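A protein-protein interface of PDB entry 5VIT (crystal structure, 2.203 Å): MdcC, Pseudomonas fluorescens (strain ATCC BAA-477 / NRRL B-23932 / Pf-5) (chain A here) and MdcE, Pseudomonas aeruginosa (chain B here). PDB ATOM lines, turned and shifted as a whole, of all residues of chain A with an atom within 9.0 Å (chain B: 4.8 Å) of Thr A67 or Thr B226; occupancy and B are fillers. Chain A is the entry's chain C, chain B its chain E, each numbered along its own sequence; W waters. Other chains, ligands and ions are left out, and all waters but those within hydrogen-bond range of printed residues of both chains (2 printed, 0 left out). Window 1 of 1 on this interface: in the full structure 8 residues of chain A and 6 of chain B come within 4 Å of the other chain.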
ATOM      1  N   PHE A   8     -18.575  -0.341   2.442  1.00  0.00           N
ATOM      2  CA  PHE A   8     -18.896  -1.705   2.089  1.00  0.00           C
ATOM      3  C   PHE A   8     -20.315  -1.777   1.618  1.00  0.00           C
ATOM      4  O   PHE A   8     -21.135  -0.948   2.014  1.00  0.00           O
ATOM      5  CB  PHE A   8     -18.673  -2.647   3.281  1.00  0.00           C
ATOM      6  CG  PHE A   8     -17.237  -2.780   3.661  1.00  0.00           C
ATOM      7  CD1 PHE A   8     -16.699  -2.000   4.672  1.00  0.00           C
ATOM      8  CD2 PHE A   8     -16.408  -3.652   2.969  1.00  0.00           C
ATOM      9  CE1 PHE A   8     -15.372  -2.105   4.996  1.00  0.00           C
ATOM     10  CE2 PHE A   8     -15.076  -3.761   3.297  1.00  0.00           C
ATOM     11  CZ  PHE A   8     -14.558  -2.984   4.305  1.00  0.00           C
ATOM     12  N   PRO A   9     -20.607  -2.765   0.756  1.00  0.00           N
ATOM     13  CA  PRO A   9     -21.986  -3.022   0.335  1.00  0.00           C
ATOM     14  C   PRO A   9     -22.812  -3.484   1.522  1.00  0.00           C
ATOM     15  O   PRO A   9     -22.359  -4.337   2.287  1.00  0.00           O
ATOM     16  CB  PRO A   9     -21.837  -4.128  -0.717  1.00  0.00           C
ATOM     17  CG  PRO A   9     -20.541  -4.799  -0.371  1.00  0.00           C
ATOM     18  CD  PRO A   9     -19.652  -3.689   0.120  1.00  0.00           C
ATOM     19  N   ALA A  10     -24.002  -2.920   1.682  1.00  0.00           N
ATOM     20  CA  ALA A  10     -24.865  -3.295   2.798  1.00  0.00           C
ATOM     21  C   ALA A  10     -26.323  -3.400   2.351  1.00  0.00           C
ATOM     22  O   ALA A  10     -26.646  -3.146   1.200  1.00  0.00           O
ATOM     23  CB  ALA A  10     -24.721  -2.296   3.937  1.00  0.00           C
ATOM     24  N   GLY A  11     -27.193  -3.795   3.266  1.00  0.00           N
ATOM     25  CA  GLY A  11     -28.597  -3.966   2.956  1.00  0.00           C
ATOM     26  C   GLY A  11     -29.392  -2.745   3.364  1.00  0.00           C
ATOM     27  O   GLY A  11     -29.003  -1.612   3.069  1.00  0.00           O
ATOM     28  N   GLN A  12     -30.505  -2.985   4.048  1.00  0.00           N
ATOM     29  CA  GLN A  12     -31.399  -1.925   4.490  1.00  0.00           C
ATOM     30  C   GLN A  12     -30.831  -1.268   5.748  1.00  0.00           C
ATOM     31  O   GLN A  12     -30.074  -1.896   6.489  1.00  0.00           O
ATOM     32  CB  GLN A  12     -32.800  -2.499   4.742  1.00  0.00           C
ATOM     33  CG  GLN A  12     -33.923  -1.863   3.925  1.00  0.00           C
ATOM     34  CD  GLN A  12     -33.572  -1.622   2.458  1.00  0.00           C
ATOM     35  OE1 GLN A  12     -33.064  -0.559   2.094  1.00  0.00           O
ATOM     36  NE2 GLN A  12     -33.862  -2.596   1.611  1.00  0.00           N
ATOM     37  N   PRO A  37     -29.155   3.145   2.705  1.00  0.00           N
ATOM     38  CA  PRO A  37     -29.402   1.799   2.153  1.00  0.00           C
ATOM     39  C   PRO A  37     -28.384   1.375   1.082  1.00  0.00           C
ATOM     40  O   PRO A  37     -27.946   2.205   0.279  1.00  0.00           O
ATOM     41  CB  PRO A  37     -30.821   1.906   1.567  1.00  0.00           C
ATOM     42  CG  PRO A  37     -31.195   3.357   1.654  1.00  0.00           C
ATOM     43  CD  PRO A  37     -30.378   3.960   2.739  1.00  0.00           C
ATOM     44  N   GLY A  38     -27.990   0.099   1.111  1.00  0.00           N
ATOM     45  CA  GLY A  38     -26.970  -0.410   0.218  1.00  0.00           C
ATOM     46  C   GLY A  38     -25.529  -0.113   0.624  1.00  0.00           C
ATOM     47  O   GLY A  38     -24.591  -0.627   0.005  1.00  0.00           O
ATOM     48  N   LYS A  39     -25.345   0.700   1.665  1.00  0.00           N
ATOM     49  CA  LYS A  39     -24.016   1.198   2.005  1.00  0.00           C
ATOM     50  C   LYS A  39     -23.685   1.176   3.511  1.00  0.00           C
ATOM     51  O   LYS A  39     -24.497   1.545   4.359  1.00  0.00           O
ATOM     52  CB  LYS A  39     -23.864   2.618   1.469  1.00  0.00           C
ATOM     53  CG  LYS A  39     -22.440   3.062   1.314  1.00  0.00           C
ATOM     54  CD  LYS A  39     -22.362   4.536   0.941  1.00  0.00           C
ATOM     55  CE  LYS A  39     -23.023   4.812  -0.390  1.00  0.00           C
ATOM     56  NZ  LYS A  39     -22.791   6.225  -0.792  1.00  0.00           N
ATOM     57  N   LEU A  40     -22.481   0.730   3.831  1.00  0.00           N
ATOM     58  CA  LEU A  40     -21.978   0.765   5.196  1.00  0.00           C
ATOM     59  C   LEU A  40     -20.740   1.632   5.218  1.00  0.00           C
ATOM     60  O   LEU A  40     -19.729   1.277   4.601  1.00  0.00           O
ATOM     61  CB  LEU A  40     -21.645  -0.633   5.695  1.00  0.00           C
ATOM     62  CG  LEU A  40     -20.982  -0.731   7.068  1.00  0.00           C
ATOM     63  CD1 LEU A  40     -21.999  -0.570   8.184  1.00  0.00           C
ATOM     64  CD2 LEU A  40     -20.277  -2.060   7.191  1.00  0.00           C
ATOM     65  N   LEU A  62     -15.098  -9.834   8.418  1.00  0.00           N
ATOM     66  CA  LEU A  62     -16.327  -9.626   9.144  1.00  0.00           C
ATOM     67  C   LEU A  62     -17.544  -9.654   8.191  1.00  0.00           C
ATOM     68  O   LEU A  62     -18.581 -10.236   8.509  1.00  0.00           O
ATOM     69  CB  LEU A  62     -16.230  -8.306   9.903  1.00  0.00           C
ATOM     70  CG  LEU A  62     -17.237  -8.021  10.999  1.00  0.00           C
ATOM     71  CD1 LEU A  62     -17.165  -9.083  12.095  1.00  0.00           C
ATOM     72  CD2 LEU A  62     -16.981  -6.614  11.536  1.00  0.00           C
ATOM     73  N   PHE A  63     -17.404  -9.053   7.013  1.00  0.00           N
ATOM     74  CA  PHE A  63     -18.541  -8.917   6.097  1.00  0.00           C
ATOM     75  C   PHE A  63     -18.531  -9.903   4.912  1.00  0.00           C
ATOM     76  O   PHE A  63     -19.329  -9.773   3.981  1.00  0.00           O
ATOM     77  CB  PHE A  63     -18.601  -7.475   5.577  1.00  0.00           C
ATOM     78  CG  PHE A  63     -18.601  -6.447   6.673  1.00  0.00           C
ATOM     79  CD1 PHE A  63     -17.806  -5.313   6.584  1.00  0.00           C
ATOM     80  CD2 PHE A  63     -19.390  -6.623   7.801  1.00  0.00           C
ATOM     81  CE1 PHE A  63     -17.792  -4.379   7.608  1.00  0.00           C
ATOM     82  CE2 PHE A  63     -19.382  -5.692   8.823  1.00  0.00           C
ATOM     83  CZ  PHE A  63     -18.581  -4.571   8.728  1.00  0.00           C
ATOM     84  N   ASP A  64     -17.643 -10.893   4.969  1.00  0.00           N
ATOM     85  CA  ASP A  64     -17.500 -11.902   3.913  1.00  0.00           C
ATOM     86  C   ASP A  64     -18.762 -12.761   3.750  1.00  0.00           C
ATOM     87  O   ASP A  64     -19.065 -13.617   4.585  1.00  0.00           O
ATOM     88  CB  ASP A  64     -16.272 -12.784   4.216  1.00  0.00           C
ATOM     89  CG  ASP A  64     -15.979 -13.822   3.124  1.00  0.00           C
ATOM     90  OD1 ASP A  64     -14.981 -14.564   3.260  1.00  0.00           O
ATOM     91  OD2 ASP A  64     -16.727 -13.912   2.133  1.00  0.00           O
ATOM     92  N   GLY A  65     -19.493 -12.528   2.663  1.00  0.00           N
ATOM     93  CA  GLY A  65     -20.650 -13.338   2.320  1.00  0.00           C
ATOM     94  C   GLY A  65     -21.831 -13.099   3.243  1.00  0.00           C
ATOM     95  O   GLY A  65     -22.735 -13.935   3.355  1.00  0.00           O
ATOM     96  N   GLN A  66     -21.830 -11.956   3.923  1.00  0.00           N
ATOM     97  CA  GLN A  66     -22.948 -11.628   4.792  1.00  0.00           C
ATOM     98  C   GLN A  66     -23.162 -10.138   4.826  1.00  0.00           C
ATOM     99  O   GLN A  66     -22.378  -9.392   5.422  1.00  0.00           O
ATOM    100  CB  GLN A  66     -22.735 -12.172   6.198  1.00  0.00           C
ATOM    101  CG  GLN A  66     -21.318 -12.120   6.663  1.00  0.00           C
ATOM    102  CD  GLN A  66     -21.074 -13.080   7.817  1.00  0.00           C
ATOM    103  OE1 GLN A  66     -21.595 -12.893   8.920  1.00  0.00           O
ATOM    104  NE2 GLN A  66     -20.295 -14.128   7.560  1.00  0.00           N
ATOM    105  N   THR A  67     -24.239  -9.726   4.171  1.00  0.00           N
ATOM    106  CA  THR A  67     -24.584  -8.325   4.021  1.00  0.00           C
ATOM    107  C   THR A  67     -25.063  -7.768   5.363  1.00  0.00           C
ATOM    108  O   THR A  67     -26.131  -8.134   5.849  1.00  0.00           O
ATOM    109  CB  THR A  67     -25.681  -8.138   2.927  1.00  0.00           C
ATOM    110  OG1 THR A  67     -25.330  -8.885   1.751  1.00  0.00           O
ATOM    111  CG2 THR A  67     -25.816  -6.690   2.552  1.00  0.00           C
ATOM    112  N   PRO A  68     -24.254  -6.893   5.973  1.00  0.00           N
ATOM    113  CA  PRO A  68     -24.651  -6.254   7.228  1.00  0.00           C
ATOM    114  C   PRO A  68     -25.759  -5.232   6.979  1.00  0.00           C
ATOM    115  O   PRO A  68     -26.038  -4.903   5.826  1.00  0.00           O
ATOM    116  CB  PRO A  68     -23.361  -5.573   7.689  1.00  0.00           C
ATOM    117  CG  PRO A  68     -22.674  -5.217   6.414  1.00  0.00           C
ATOM    118  CD  PRO A  68     -22.988  -6.342   5.452  1.00  0.00           C
ATOM    119  N   PRO A  69     -26.398  -4.749   8.046  1.00  0.00           N
ATOM    120  CA  PRO A  69     -27.324  -3.632   7.869  1.00  0.00           C
ATOM    121  C   PRO A  69     -26.563  -2.385   7.436  1.00  0.00           C
ATOM    122  O   PRO A  69     -25.373  -2.257   7.741  1.00  0.00           O
ATOM    123  CB  PRO A  69     -27.940  -3.467   9.261  1.00  0.00           C
ATOM    124  CG  PRO A  69     -26.924  -4.055  10.194  1.00  0.00           C
ATOM    125  CD  PRO A  69     -26.363  -5.219   9.443  1.00  0.00           C
ATOM    126  N   ALA A  70     -27.223  -1.499   6.703  1.00  0.00           N
ATOM    127  CA  ALA A  70     -26.608  -0.240   6.320  1.00  0.00           C
ATOM    128  C   ALA A  70     -26.495   0.626   7.568  1.00  0.00           C
ATOM    129  O   ALA A  70     -27.495   1.001   8.176  1.00  0.00           O
ATOM    130  CB  ALA A  70     -27.417   0.461   5.226  1.00  0.00           C
ATOM    131  N   PHE A  93     -22.868  -4.782  16.621  1.00  0.00           N
ATOM    132  CA  PHE A  93     -23.855  -5.281  15.651  1.00  0.00           C
ATOM    133  C   PHE A  93     -24.963  -6.057  16.337  1.00  0.00           C
ATOM    134  O   PHE A  93     -26.114  -5.996  15.908  1.00  0.00           O
ATOM    135  CB  PHE A  93     -23.190  -6.161  14.584  1.00  0.00           C
ATOM    136  CG  PHE A  93     -22.583  -5.380  13.443  1.00  0.00           C
ATOM    137  CD1 PHE A  93     -21.220  -5.108  13.413  1.00  0.00           C
ATOM    138  CD2 PHE A  93     -23.376  -4.908  12.404  1.00  0.00           C
ATOM    139  CE1 PHE A  93     -20.654  -4.393  12.364  1.00  0.00           C
ATOM    140  CE2 PHE A  93     -22.818  -4.190  11.357  1.00  0.00           C
ATOM    141  CZ  PHE A  93     -21.455  -3.930  11.334  1.00  0.00           C
ATOM    142  N   ALA B 173     -29.714 -11.629  -3.898  1.00  0.00           N
ATOM    143  CA  ALA B 173     -31.105 -11.229  -3.935  1.00  0.00           C
ATOM    144  C   ALA B 173     -31.189  -9.702  -3.971  1.00  0.00           C
ATOM    145  O   ALA B 173     -30.390  -9.019  -3.318  1.00  0.00           O
ATOM    146  CB  ALA B 173     -31.863 -11.791  -2.730  1.00  0.00           C
ATOM    147  N   HIS B 175     -32.761  -6.507  -2.588  1.00  0.00           N
ATOM    148  CA  HIS B 175     -33.436  -6.297  -1.313  1.00  0.00           C
ATOM    149  C   HIS B 175     -34.748  -5.544  -1.497  1.00  0.00           C
ATOM    150  O   HIS B 175     -34.818  -4.326  -1.302  1.00  0.00           O
ATOM    151  CB  HIS B 175     -32.540  -5.553  -0.315  1.00  0.00           C
ATOM    152  CG  HIS B 175     -32.917  -5.811   1.113  1.00  0.00           C
ATOM    153  ND1 HIS B 175     -34.218  -5.732   1.561  1.00  0.00           N
ATOM    154  CD2 HIS B 175     -32.171  -6.180   2.185  1.00  0.00           C
ATOM    155  CE1 HIS B 175     -34.257  -6.021   2.852  1.00  0.00           C
ATOM    156  NE2 HIS B 175     -33.029  -6.293   3.255  1.00  0.00           N
ATOM    157  N   ALA B 218     -32.225 -14.252   4.375  1.00  0.00           N
ATOM    158  CA  ALA B 218     -30.831 -13.870   4.548  1.00  0.00           C
ATOM    159  C   ALA B 218     -30.269 -14.422   5.858  1.00  0.00           C
ATOM    160  O   ALA B 218     -29.117 -14.845   5.916  1.00  0.00           O
ATOM    161  CB  ALA B 218     -30.681 -12.350   4.517  1.00  0.00           C
ATOM    162  N   LEU B 223     -27.674 -16.493   1.307  1.00  0.00           N
ATOM    163  CA  LEU B 223     -27.337 -15.478   0.303  1.00  0.00           C
ATOM    164  C   LEU B 223     -25.915 -14.965   0.486  1.00  0.00           C
ATOM    165  O   LEU B 223     -25.464 -14.756   1.621  1.00  0.00           O
ATOM    166  CB  LEU B 223     -28.308 -14.299   0.366  1.00  0.00           C
ATOM    167  CG  LEU B 223     -29.785 -14.612   0.161  1.00  0.00           C
ATOM    168  CD1 LEU B 223     -30.665 -13.411   0.515  1.00  0.00           C
ATOM    169  CD2 LEU B 223     -30.003 -15.057  -1.269  1.00  0.00           C
ATOM    170  N   TRP B 224     -25.216 -14.765  -0.630  1.00  0.00           N
ATOM    171  CA  TRP B 224     -23.868 -14.206  -0.600  1.00  0.00           C
ATOM    172  C   TRP B 224     -23.945 -12.684  -0.461  1.00  0.00           C
ATOM    173  O   TRP B 224     -23.123 -12.065   0.212  1.00  0.00           O
ATOM    174  CB  TRP B 224     -23.082 -14.587  -1.862  1.00  0.00           C
ATOM    175  CG  TRP B 224     -21.668 -14.031  -1.882  1.00  0.00           C
ATOM    176  CD1 TRP B 224     -20.615 -14.439  -1.111  1.00  0.00           C
ATOM    177  CD2 TRP B 224     -21.166 -12.979  -2.714  1.00  0.00           C
ATOM    178  NE1 TRP B 224     -19.493 -13.700  -1.404  1.00  0.00           N
ATOM    179  CE2 TRP B 224     -19.799 -12.803  -2.391  1.00  0.00           C
ATOM    180  CE3 TRP B 224     -21.737 -12.166  -3.706  1.00  0.00           C
ATOM    181  CZ2 TRP B 224     -18.993 -11.846  -3.019  1.00  0.00           C
ATOM    182  CZ3 TRP B 224     -20.931 -11.216  -4.334  1.00  0.00           C
ATOM    183  CH2 TRP B 224     -19.570 -11.070  -3.987  1.00  0.00           C
ATOM    184  N   ARG B 225     -24.943 -12.094  -1.106  1.00  0.00           N
ATOM    185  CA  ARG B 225     -25.223 -10.680  -0.937  1.00  0.00           C
ATOM    186  C   ARG B 225     -26.694 -10.346  -1.180  1.00  0.00           C
ATOM    187  O   ARG B 225     -27.386 -11.019  -1.944  1.00  0.00           O
ATOM    188  CB  ARG B 225     -24.351  -9.834  -1.865  1.00  0.00           C
ATOM    189  CG  ARG B 225     -24.260  -8.394  -1.389  1.00  0.00           C
ATOM    190  CD  ARG B 225     -23.185  -7.593  -2.099  1.00  0.00           C
ATOM    191  NE  ARG B 225     -21.844  -8.133  -1.896  1.00  0.00           N
ATOM    192  CZ  ARG B 225     -20.776  -7.727  -2.583  1.00  0.00           C
ATOM    193  NH1 ARG B 225     -20.909  -6.778  -3.509  1.00  0.00           N
ATOM    194  NH2 ARG B 225     -19.579  -8.261  -2.341  1.00  0.00           N
ATOM    195  N   THR B 226     -27.164  -9.311  -0.499  1.00  0.00           N
ATOM    196  CA  THR B 226     -28.406  -8.658  -0.875  1.00  0.00           C
ATOM    197  C   THR B 226     -28.079  -7.242  -1.337  1.00  0.00           C
ATOM    198  O   THR B 226     -27.135  -6.617  -0.853  1.00  0.00           O
ATOM    199  CB  THR B 226     -29.418  -8.584   0.277  1.00  0.00           C
ATOM    200  OG1 THR B 226     -28.956  -7.635   1.244  1.00  0.00           O
ATOM    201  CG2 THR B 226     -29.601  -9.945   0.922  1.00  0.00           C
ATOM    202  N   LEU B 227     -28.846  -6.723  -2.279  1.00  0.00           N
ATOM    203  CA  LEU B 227     -28.609  -5.346  -2.652  1.00  0.00           C
ATOM    204  C   LEU B 227     -29.898  -4.660  -3.030  1.00  0.00           C
ATOM    205  O   LEU B 227     -30.648  -5.136  -3.886  1.00  0.00           O
ATOM    206  CB  LEU B 227     -27.569  -5.260  -3.770  1.00  0.00           C
ATOM    207  CG  LEU B 227     -27.814  -5.891  -5.122  1.00  0.00           C
ATOM    208  CD1 LEU B 227     -28.322  -4.801  -6.055  1.00  0.00           C
ATOM    209  CD2 LEU B 227     -26.522  -6.508  -5.648  1.00  0.00           C
ATOM    210  N   PRO B 228     -30.183  -3.556  -2.330  1.00  0.00           N
ATOM    211  CA  PRO B 228     -31.349  -2.722  -2.621  1.00  0.00           C
ATOM    212  C   PRO B 228     -31.150  -1.963  -3.923  1.00  0.00           C
ATOM    213  O   PRO B 228     -30.028  -1.594  -4.267  1.00  0.00           O
ATOM    214  CB  PRO B 228     -31.436  -1.772  -1.418  1.00  0.00           C
ATOM    215  CG  PRO B 228     -30.150  -1.885  -0.694  1.00  0.00           C
ATOM    216  CD  PRO B 228     -29.506  -3.184  -1.073  1.00  0.00           C
HETATM  217  O   HOH W   1     -16.884 -13.373  -0.252  1.00  0.00           O
HETATM  218  O   HOH W   2     -25.555  -4.107  -0.991  1.00  0.00           O
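The backbone carbonyl oxygen (O) of Gly A65 sits close to the backbone carbonyl oxygen (O) of Leu B223 (3.3 Å).
The backbone NH of Thr B226 sits at hydrogen-bond distance from the side-chain hydroxyl of Thr A67 (2.9 Å).
NE2 of Gln A12 is in hydrogen-bond range of ND1 of His B175 (3.2 Å).
The backbone carbonyl oxygen (O) of Pro A68 is in hydrogen-bond range of the backbone NH (N) of Gly A11 (3.0 Å).
O of Asp A64 is in hydrogen-bond range of NE2 of Gln A66, at 3.3 Å.
The backbone carbonyl oxygen of Gly A11 lies within hydrogen-bond range of the backbone NH of Gly A38, 2.8 Å away.
N of Ala A10 sits at hydrogen-bond distance from O of Gly A38, at 2.9 Å.
The backbone NH of Ala B173 is in hydrogen-bond range of the backbone carbonyl oxygen of Arg B225 (3.1 Å).
The backbone carbonyl oxygen (O) of Gln A12 sits at hydrogen-bond distance from the backbone NH (N) of Ala A70 (2.9 Å).
Among the printed residues, merely in contact across the chains: Thr A67 with Arg B225 (3.2 Å), Gly A38 with Pro B228 (3.4 Å), Gly A65 with Trp B224 (3.5 Å), Ala A10 with Pro B228 (3.7 Å), Pro A9 with Arg B225 (3.7 Å), Gln A66 with Trp B224 (3.9 Å), Gly A11 with Pro B228 (3.9 Å) and Gln A12 with Pro B228 (3.97 Å).
Of chain B, only Arg B225 and Thr B226 come within 4 Å of Thr A67.
Thr B226 touches one residue of chain A.
Of the printed residues of chain A, Arg B225 touches Pro A9 (3.7 Å) and Thr A67 (3.2 Å).
Of the printed residues of chain A, Trp B224 touches Gly A65 and Gln A66.
Of the printed residues of chain B, Gln A12 touches His B175 and Pro B228.
Of the printed residues of chain B, Gly A11 touches Pro B228 (3.9 Å).
Of the printed residues of chain B, Gly A38 touches Pro B228 (3.4 Å).
Lys A39 touches none of the printed residues of chain B.
Pro A37 touches none of the printed residues of chain B.
Of the 19 printed residues of chain A, 8 touch a printed residue of chain B.
Hydrophobic or aromatic side chains of chain A within 4 Å of the printed part of chain B: Pro A9.
Along chain A the printed residues that touch a printed residue of chain B span positions 9 to 67.
Among the printed residues, 11 pairs touch across the chains.
Water W1 lies within hydrogen-bond range of OD2 of Asp A64 and NE1 of Trp B224.
Water W2 bridges O of Ala A10 (2.6 Å) and O of Thr B226 (3.0 Å).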
